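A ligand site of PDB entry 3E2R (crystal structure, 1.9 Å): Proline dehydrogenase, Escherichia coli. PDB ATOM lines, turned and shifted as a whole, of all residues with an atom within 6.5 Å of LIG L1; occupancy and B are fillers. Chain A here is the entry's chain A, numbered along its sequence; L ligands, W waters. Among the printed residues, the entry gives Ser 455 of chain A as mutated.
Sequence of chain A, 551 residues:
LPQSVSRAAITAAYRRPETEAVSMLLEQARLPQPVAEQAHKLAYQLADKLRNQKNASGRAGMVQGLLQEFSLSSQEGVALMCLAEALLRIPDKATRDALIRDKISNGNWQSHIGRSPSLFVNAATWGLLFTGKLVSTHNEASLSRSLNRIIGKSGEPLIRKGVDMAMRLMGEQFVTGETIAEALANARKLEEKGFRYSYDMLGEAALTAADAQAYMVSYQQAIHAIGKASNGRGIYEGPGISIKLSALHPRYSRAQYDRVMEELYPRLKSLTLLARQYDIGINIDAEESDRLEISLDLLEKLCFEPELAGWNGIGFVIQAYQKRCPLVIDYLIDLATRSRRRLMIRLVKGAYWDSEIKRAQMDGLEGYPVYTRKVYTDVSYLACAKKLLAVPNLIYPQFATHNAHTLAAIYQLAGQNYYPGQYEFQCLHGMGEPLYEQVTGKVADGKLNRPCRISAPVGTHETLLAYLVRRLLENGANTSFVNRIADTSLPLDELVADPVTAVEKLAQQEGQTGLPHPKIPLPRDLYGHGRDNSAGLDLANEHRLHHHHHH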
ATOM      1  N   ASP A 200     -11.074 -18.671  -5.535  1.00  0.00           N
ATOM      2  CA  ASP A 200     -10.890 -18.924  -4.125  1.00  0.00           C
ATOM      3  C   ASP A 200     -12.218 -18.625  -3.436  1.00  0.00           C
ATOM      4  O   ASP A 200     -12.631 -17.470  -3.357  1.00  0.00           O
ATOM      5  CB  ASP A 200      -9.763 -18.066  -3.568  1.00  0.00           C
ATOM      6  CG  ASP A 200      -9.230 -18.591  -2.241  1.00  0.00           C
ATOM      7  OD1 ASP A 200      -8.003 -18.756  -2.110  1.00  0.00           O
ATOM      8  OD2 ASP A 200     -10.054 -18.848  -1.337  1.00  0.00           O
ATOM      9  N   GLU A 204     -14.340 -19.324   5.562  1.00  0.00           N
ATOM     10  CA  GLU A 204     -13.212 -19.915   6.257  1.00  0.00           C
ATOM     11  C   GLU A 204     -13.602 -20.134   7.710  1.00  0.00           C
ATOM     12  O   GLU A 204     -14.663 -19.686   8.143  1.00  0.00           O
ATOM     13  CB  GLU A 204     -12.004 -18.983   6.172  1.00  0.00           C
ATOM     14  CG  GLU A 204     -12.235 -17.596   6.770  1.00  0.00           C
ATOM     15  CD  GLU A 204     -11.108 -16.631   6.482  1.00  0.00           C
ATOM     16  OE1 GLU A 204     -10.908 -16.257   5.298  1.00  0.00           O
ATOM     17  OE2 GLU A 204     -10.404 -16.243   7.431  1.00  0.00           O
ATOM     18  N   SER A 242      -8.932 -22.802  -5.406  1.00  0.00           N
ATOM     19  CA  SER A 242      -8.095 -22.654  -4.232  1.00  0.00           C
ATOM     20  C   SER A 242      -8.956 -22.890  -3.010  1.00  0.00           C
ATOM     21  O   SER A 242     -10.077 -22.379  -2.926  1.00  0.00           O
ATOM     22  CB  SER A 242      -7.504 -21.241  -4.186  1.00  0.00           C
ATOM     23  OG  SER A 242      -6.212 -21.260  -3.623  1.00  0.00           O
ATOM     24  N   LYS A 244      -9.441 -23.503   1.424  1.00  0.00           N
ATOM     25  CA  LYS A 244      -8.955 -23.263   2.778  1.00  0.00           C
ATOM     26  C   LYS A 244      -9.315 -24.460   3.650  1.00  0.00           C
ATOM     27  O   LYS A 244     -10.490 -24.805   3.781  1.00  0.00           O
ATOM     28  CB  LYS A 244      -9.532 -21.966   3.352  1.00  0.00           C
ATOM     29  CG  LYS A 244      -8.802 -20.692   2.881  1.00  0.00           C
ATOM     30  CD  LYS A 244      -9.430 -19.429   3.461  1.00  0.00           C
ATOM     31  CE  LYS A 244      -8.497 -18.217   3.342  1.00  0.00           C
ATOM     32  NZ  LYS A 244      -8.145 -17.889   1.918  1.00  0.00           N
ATOM     33  N   ASP A 285      -4.575 -23.178   0.282  1.00  0.00           N
ATOM     34  CA  ASP A 285      -4.184 -21.900   0.889  1.00  0.00           C
ATOM     35  C   ASP A 285      -3.476 -22.130   2.205  1.00  0.00           C
ATOM     36  O   ASP A 285      -3.732 -23.122   2.897  1.00  0.00           O
ATOM     37  CB  ASP A 285      -5.407 -21.014   1.142  1.00  0.00           C
ATOM     38  CG  ASP A 285      -5.992 -20.428  -0.115  1.00  0.00           C
ATOM     39  OD1 ASP A 285      -5.420 -20.642  -1.208  1.00  0.00           O
ATOM     40  OD2 ASP A 285      -7.041 -19.752  -0.014  1.00  0.00           O
ATOM     41  N   ALA A 286      -2.597 -21.204   2.558  1.00  0.00           N
ATOM     42  CA  ALA A 286      -1.897 -21.248   3.824  1.00  0.00           C
ATOM     43  C   ALA A 286      -2.602 -20.284   4.773  1.00  0.00           C
ATOM     44  O   ALA A 286      -2.920 -19.149   4.396  1.00  0.00           O
ATOM     45  CB  ALA A 286      -0.444 -20.859   3.633  1.00  0.00           C
ATOM     46  N   VAL A 317       0.448 -23.455  -0.847  1.00  0.00           N
ATOM     47  CA  VAL A 317       1.012 -22.135  -0.557  1.00  0.00           C
ATOM     48  C   VAL A 317       2.043 -22.234   0.546  1.00  0.00           C
ATOM     49  O   VAL A 317       1.868 -22.978   1.511  1.00  0.00           O
ATOM     50  CB  VAL A 317      -0.082 -21.145  -0.067  1.00  0.00           C
ATOM     51  CG1 VAL A 317       0.563 -19.809   0.352  1.00  0.00           C
ATOM     52  CG2 VAL A 317      -1.115 -20.914  -1.139  1.00  0.00           C
ATOM     53  N   ARG A 346       2.859 -22.053  -4.530  1.00  0.00           N
ATOM     54  CA  ARG A 346       2.676 -20.604  -4.518  1.00  0.00           C
ATOM     55  C   ARG A 346       3.531 -20.011  -3.419  1.00  0.00           C
ATOM     56  O   ARG A 346       3.300 -20.286  -2.237  1.00  0.00           O
ATOM     57  CB  ARG A 346       1.218 -20.239  -4.251  1.00  0.00           C
ATOM     58  CG  ARG A 346       0.268 -20.772  -5.289  1.00  0.00           C
ATOM     59  CD  ARG A 346      -1.135 -20.203  -5.103  1.00  0.00           C
ATOM     60  NE  ARG A 346      -2.041 -20.754  -6.101  1.00  0.00           N
ATOM     61  CZ  ARG A 346      -3.331 -20.439  -6.192  1.00  0.00           C
ATOM     62  NH1 ARG A 346      -3.866 -19.576  -5.317  1.00  0.00           N
ATOM     63  NH2 ARG A 346      -4.082 -20.995  -7.135  1.00  0.00           N
ATOM     64  N   ALA A 351      -0.626 -13.299   4.681  1.00  0.00           N
ATOM     65  CA  ALA A 351      -1.773 -12.406   4.848  1.00  0.00           C
ATOM     66  C   ALA A 351      -2.180 -12.126   6.291  1.00  0.00           C
ATOM     67  O   ALA A 351      -3.058 -11.285   6.555  1.00  0.00           O
ATOM     68  CB  ALA A 351      -2.967 -12.944   4.049  1.00  0.00           C
ATOM     69  N   TYR A 352      -1.560 -12.813   7.249  1.00  0.00           N
ATOM     70  CA  TYR A 352      -2.069 -12.780   8.621  1.00  0.00           C
ATOM     71  C   TYR A 352      -1.112 -12.126   9.604  1.00  0.00           C
ATOM     72  O   TYR A 352      -1.187 -12.376  10.799  1.00  0.00           O
ATOM     73  CB  TYR A 352      -2.358 -14.215   9.108  1.00  0.00           C
ATOM     74  CG  TYR A 352      -3.334 -14.950   8.223  1.00  0.00           C
ATOM     75  CD1 TYR A 352      -4.680 -15.054   8.562  1.00  0.00           C
ATOM     76  CD2 TYR A 352      -2.907 -15.565   7.039  1.00  0.00           C
ATOM     77  CE1 TYR A 352      -5.577 -15.752   7.744  1.00  0.00           C
ATOM     78  CE2 TYR A 352      -3.784 -16.251   6.228  1.00  0.00           C
ATOM     79  CZ  TYR A 352      -5.112 -16.336   6.581  1.00  0.00           C
ATOM     80  OH  TYR A 352      -5.974 -17.025   5.736  1.00  0.00           O
ATOM     81  N   LEU A 428      -3.808 -10.716  -6.590  1.00  0.00           N
ATOM     82  CA  LEU A 428      -5.189 -10.749  -6.091  1.00  0.00           C
ATOM     83  C   LEU A 428      -6.058  -9.853  -6.954  1.00  0.00           C
ATOM     84  O   LEU A 428      -5.653  -8.759  -7.333  1.00  0.00           O
ATOM     85  CB  LEU A 428      -5.253 -10.279  -4.619  1.00  0.00           C
ATOM     86  CG  LEU A 428      -4.452 -11.028  -3.549  1.00  0.00           C
ATOM     87  CD1 LEU A 428      -4.714 -10.427  -2.148  1.00  0.00           C
ATOM     88  CD2 LEU A 428      -4.807 -12.508  -3.575  1.00  0.00           C
ATOM     89  N   SER A 455      -6.045 -14.450  -8.418  1.00  0.00           N
ATOM     90  CA  SER A 455      -6.839 -15.106  -7.400  1.00  0.00           C
ATOM     91  C   SER A 455      -8.158 -14.354  -7.294  1.00  0.00           C
ATOM     92  O   SER A 455      -8.175 -13.149  -7.045  1.00  0.00           O
ATOM     93  CB  SER A 455      -6.107 -15.129  -6.050  1.00  0.00           C
ATOM     94  OG  SER A 455      -6.899 -15.739  -5.046  1.00  0.00           O
ATOM     95  N   ALA A 466     -13.623 -11.655   6.937  1.00  0.00           N
ATOM     96  CA  ALA A 466     -12.218 -11.851   7.290  1.00  0.00           C
ATOM     97  C   ALA A 466     -11.278 -11.527   6.129  1.00  0.00           C
ATOM     98  O   ALA A 466     -10.220 -10.934   6.322  1.00  0.00           O
ATOM     99  CB  ALA A 466     -11.978 -13.272   7.803  1.00  0.00           C
ATOM    100  N   TYR A 467     -11.675 -11.918   4.921  1.00  0.00           N
ATOM    101  CA  TYR A 467     -10.865 -11.626   3.733  1.00  0.00           C
ATOM    102  C   TYR A 467     -10.706 -10.118   3.549  1.00  0.00           C
ATOM    103  O   TYR A 467      -9.606  -9.608   3.303  1.00  0.00           O
ATOM    104  CB  TYR A 467     -11.516 -12.231   2.484  1.00  0.00           C
ATOM    105  CG  TYR A 467     -10.685 -12.112   1.212  1.00  0.00           C
ATOM    106  CD1 TYR A 467      -9.735 -13.070   0.894  1.00  0.00           C
ATOM    107  CD2 TYR A 467     -10.863 -11.049   0.340  1.00  0.00           C
ATOM    108  CE1 TYR A 467      -8.971 -12.972  -0.264  1.00  0.00           C
ATOM    109  CE2 TYR A 467     -10.096 -10.940  -0.827  1.00  0.00           C
ATOM    110  CZ  TYR A 467      -9.160 -11.901  -1.118  1.00  0.00           C
ATOM    111  OH  TYR A 467      -8.403 -11.808  -2.273  1.00  0.00           O
ATOM    112  N   ARG A 470      -8.273  -8.569   6.020  1.00  0.00           N
ATOM    113  CA  ARG A 470      -6.897  -8.792   5.576  1.00  0.00           C
ATOM    114  C   ARG A 470      -6.495  -7.855   4.429  1.00  0.00           C
ATOM    115  O   ARG A 470      -5.361  -7.352   4.405  1.00  0.00           O
ATOM    116  CB  ARG A 470      -6.653 -10.264   5.238  1.00  0.00           C
ATOM    117  CG  ARG A 470      -6.740 -11.179   6.465  1.00  0.00           C
ATOM    118  CD  ARG A 470      -6.223 -12.596   6.196  1.00  0.00           C
ATOM    119  NE  ARG A 470      -7.024 -13.316   5.199  1.00  0.00           N
ATOM    120  CZ  ARG A 470      -8.132 -14.004   5.470  1.00  0.00           C
ATOM    121  NH1 ARG A 470      -8.593 -14.072   6.725  1.00  0.00           N
ATOM    122  NH2 ARG A 470      -8.781 -14.617   4.492  1.00  0.00           N
ATOM    123  N   ARG A 471      -7.415  -7.589   3.502  1.00  0.00           N
ATOM    124  CA  ARG A 471      -7.132  -6.652   2.410  1.00  0.00           C
ATOM    125  C   ARG A 471      -6.962  -5.212   2.914  1.00  0.00           C
ATOM    126  O   ARG A 471      -6.145  -4.455   2.401  1.00  0.00           O
ATOM    127  CB  ARG A 471      -8.222  -6.713   1.331  1.00  0.00           C
ATOM    128  CG  ARG A 471      -8.407  -8.071   0.680  1.00  0.00           C
ATOM    129  CD  ARG A 471      -7.229  -8.465  -0.218  1.00  0.00           C
ATOM    130  NE  ARG A 471      -6.055  -8.984   0.491  1.00  0.00           N
ATOM    131  CZ  ARG A 471      -6.016 -10.151   1.137  1.00  0.00           C
ATOM    132  NH1 ARG A 471      -7.105 -10.902   1.221  1.00  0.00           N
ATOM    133  NH2 ARG A 471      -4.897 -10.558   1.715  1.00  0.00           N
ATOM    134  N   GLU A 474      -3.492  -5.073   4.454  1.00  0.00           N
ATOM    135  CA  GLU A 474      -2.517  -5.099   3.376  1.00  0.00           C
ATOM    136  C   GLU A 474      -2.417  -3.749   2.662  1.00  0.00           C
ATOM    137  O   GLU A 474      -1.322  -3.214   2.475  1.00  0.00           O
ATOM    138  CB  GLU A 474      -2.896  -6.203   2.376  1.00  0.00           C
ATOM    139  CG  GLU A 474      -1.819  -6.488   1.327  1.00  0.00           C
ATOM    140  CD  GLU A 474      -2.245  -7.573   0.339  1.00  0.00           C
ATOM    141  OE1 GLU A 474      -3.286  -8.221   0.560  1.00  0.00           O
ATOM    142  OE2 GLU A 474      -1.527  -7.776  -0.661  1.00  0.00           O
HETATM  143  O1  LIG L   1      -5.114 -16.415   0.990  1.00  0.00           O
HETATM  144  C1  LIG L   1      -5.071 -14.932   1.231  1.00  0.00           C
HETATM  145  C2  LIG L   1      -6.204 -14.365   2.062  1.00  0.00           C
HETATM  146  O2  LIG L   1      -6.147 -13.253   2.456  1.00  0.00           O
HETATM  147  C3  LIG L   1      -4.953 -14.387  -0.172  1.00  0.00           C
HETATM  148  C4  LIG L   1      -5.672 -15.336  -1.048  1.00  0.00           C
HETATM  149  C5  LIG L   1      -5.798 -16.605  -0.290  1.00  0.00           C
HETATM  150  O3  LIG L   1      -7.307 -15.177   2.324  1.00  0.00           O
HETATM  151  P1  LG2 L   2       4.653  -6.200  -0.171  1.00  0.00           P
HETATM  152  O1  LG2 L   2       4.166  -4.669   0.180  1.00  0.00           O
HETATM  153  O2  LG2 L   2       5.937  -6.184  -0.898  1.00  0.00           O
HETATM  154  O3  LG2 L   2       4.829  -7.033   1.207  1.00  0.00           O
HETATM  155  C1  LG2 L   2       3.643  -7.105   1.953  1.00  0.00           C
HETATM  156  C2  LG2 L   2       3.721  -7.747   3.325  1.00  0.00           C
HETATM  157  O4  LG2 L   2       4.927  -8.097   3.995  1.00  0.00           O
HETATM  158  C3  LG2 L   2       2.686  -8.459   3.979  1.00  0.00           C
HETATM  159  O5  LG2 L   2       1.461  -8.765   3.372  1.00  0.00           O
HETATM  160  C4  LG2 L   2       3.350  -9.293   4.917  1.00  0.00           C
HETATM  161  O6  LG2 L   2       3.399 -10.685   4.710  1.00  0.00           O
HETATM  162  C5  LG2 L   2       4.534  -8.576   5.218  1.00  0.00           C
HETATM  163  N1  LG2 L   2       4.784  -7.706   6.350  1.00  0.00           N
HETATM  164  C6  LG2 L   2       4.208  -6.525   6.547  1.00  0.00           C
HETATM  165  N2  LG2 L   2       4.785  -5.965   7.668  1.00  0.00           N
HETATM  166  C7  LG2 L   2       5.738  -6.834   8.125  1.00  0.00           C
HETATM  167  C8  LG2 L   2       6.587  -6.776   9.178  1.00  0.00           C
HETATM  168  N3  LG2 L   2       6.593  -5.617  10.056  1.00  0.00           N
HETATM  169  N4  LG2 L   2       7.423  -7.777   9.413  1.00  0.00           N
HETATM  170  C9  LG2 L   2       7.445  -8.865   8.600  1.00  0.00           C
HETATM  171  N5  LG2 L   2       6.586  -8.921   7.557  1.00  0.00           N
HETATM  172  C10 LG2 L   2       5.752  -7.910   7.313  1.00  0.00           C
HETATM  173  N6  LG2 L   2      -1.055 -15.165   2.095  1.00  0.00           N
HETATM  174  C11 LG2 L   2      -1.306 -16.146   2.972  1.00  0.00           C
HETATM  175  O7  LG2 L   2      -0.983 -15.988   4.323  1.00  0.00           O
HETATM  176  N7  LG2 L   2      -1.892 -17.325   2.559  1.00  0.00           N
HETATM  177  C12 LG2 L   2      -2.221 -17.490   1.241  1.00  0.00           C
HETATM  178  O8  LG2 L   2      -2.799 -18.712   0.899  1.00  0.00           O
HETATM  179  C13 LG2 L   2      -1.972 -16.505   0.305  1.00  0.00           C
HETATM  180  N8  LG2 L   2      -2.290 -16.663  -1.003  1.00  0.00           N
HETATM  181  C14 LG2 L   2      -2.042 -15.686  -1.864  1.00  0.00           C
HETATM  182  C15 LG2 L   2      -2.361 -15.806  -3.235  1.00  0.00           C
HETATM  183  C16 LG2 L   2      -2.076 -14.760  -4.109  1.00  0.00           C
HETATM  184  C17 LG2 L   2      -2.406 -14.901  -5.602  1.00  0.00           C
HETATM  185  C18 LG2 L   2      -1.486 -13.593  -3.644  1.00  0.00           C
HETATM  186  C19 LG2 L   2      -1.201 -12.415  -4.571  1.00  0.00           C
HETATM  187  C20 LG2 L   2      -1.168 -13.471  -2.302  1.00  0.00           C
HETATM  188  C21 LG2 L   2      -1.455 -14.527  -1.419  1.00  0.00           C
HETATM  189  N9  LG2 L   2      -1.140 -14.377  -0.132  1.00  0.00           N
HETATM  190  C22 LG2 L   2      -1.397 -15.353   0.739  1.00  0.00           C
HETATM  191  C23 LG2 L   2      -0.364 -13.204   0.234  1.00  0.00           C
HETATM  192  C24 LG2 L   2      -1.146 -12.042   0.802  1.00  0.00           C
HETATM  193  O9  LG2 L   2      -2.337 -12.095   0.701  1.00  0.00           O
HETATM  194  C25 LG2 L   2      -0.540 -10.693   0.467  1.00  0.00           C
HETATM  195  O10 LG2 L   2      -1.078 -10.332  -0.778  1.00  0.00           O
HETATM  196  C26 LG2 L   2       0.984 -10.594   0.423  1.00  0.00           C
HETATM  197  O11 LG2 L   2       1.675 -10.958   1.595  1.00  0.00           O
HETATM  198  C27 LG2 L   2       1.473  -9.288  -0.175  1.00  0.00           C
HETATM  199  O12 LG2 L   2       2.808  -9.321  -0.583  1.00  0.00           O
HETATM  200  P2  LG2 L   2       3.316  -8.280  -1.733  1.00  0.00           P
HETATM  201  O13 LG2 L   2       4.800  -8.734  -2.214  1.00  0.00           O
HETATM  202  O14 LG2 L   2       2.321  -8.086  -2.776  1.00  0.00           O
HETATM  203  O15 LG2 L   2       3.386  -6.794  -0.991  1.00  0.00           O
HETATM  204  O   HOH W   1      -5.277 -18.137   3.097  1.00  0.00           O
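The guanidinium group of Arg 471 sits at hydrogen-bond distance from an oxygen (O9) of LG2 L2, at 3.2 Å.
The guanidinium group (NH2) of Arg 470 lies within salt-bridge range of an oxygen (O3) of LIG L1 (2.7 Å).
An oxygen (O10) of LG2 L2 sits at hydrogen-bond distance from the side-chain carboxylate (OE2) of Glu 474, 2.6 Å away.
The side-chain amino group of Lys 244 is in salt-bridge range of an oxygen (O3) of LIG L1 (2.9 Å).
The guanidinium group (NH1) of Arg 471 lies within salt-bridge range of an oxygen (O2) of LIG L1 (2.8 Å).
O8 of LG2 L2 sits at hydrogen-bond distance from N of Ala 286, 3.0 Å away.
The backbone NH of Ala 351 sits at hydrogen-bond distance from an oxygen (O7) of LG2 L2 (2.7 Å).
The backbone carbonyl oxygen (O) of Ala 286 sits at hydrogen-bond distance from a nitrogen (N7) of LG2 L2 (2.8 Å).
The side-chain carboxylate (OD1) of Asp 200 lies close to the side-chain carboxylate (OD2) of Asp 285 (2.5 Å).
The side-chain carboxylate (OD1) of Asp 285 is in hydrogen-bond range of the side-chain hydroxyl (OG) of Ser 242 (2.6 Å).
The side-chain amino group (NZ) of Lys 244 lies within salt-bridge range of the side-chain carboxylate (OD2) of Asp 285, 2.9 Å away.
The side-chain amino group (NZ) of Lys 244 is in salt-bridge range of the side-chain carboxylate (OD2) of Asp 200 (3.9 Å).
OD1 of Asp 200 sits close to OG of Ser 242 (3.4 Å).
The guanidinium group (NH2) of Arg 470 is in salt-bridge range of the side-chain carboxylate (OE1) of Glu 204, at 2.8 Å.
The guanidinium group (NE) of Arg 471 is in salt-bridge range of the side-chain carboxylate (OE1) of Glu 474 (2.9 Å).
Merely in contact with LIG L1: Asp 200, Asp 285, Ala 351, Leu 428 and Tyr 467.
Hydrophobic or aromatic side chains that line LIG L1: Ala 351, Leu 428 and Tyr 467.
The nearest printed residue that does not touch LIG L1 is Tyr 352 (4.1 Å).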
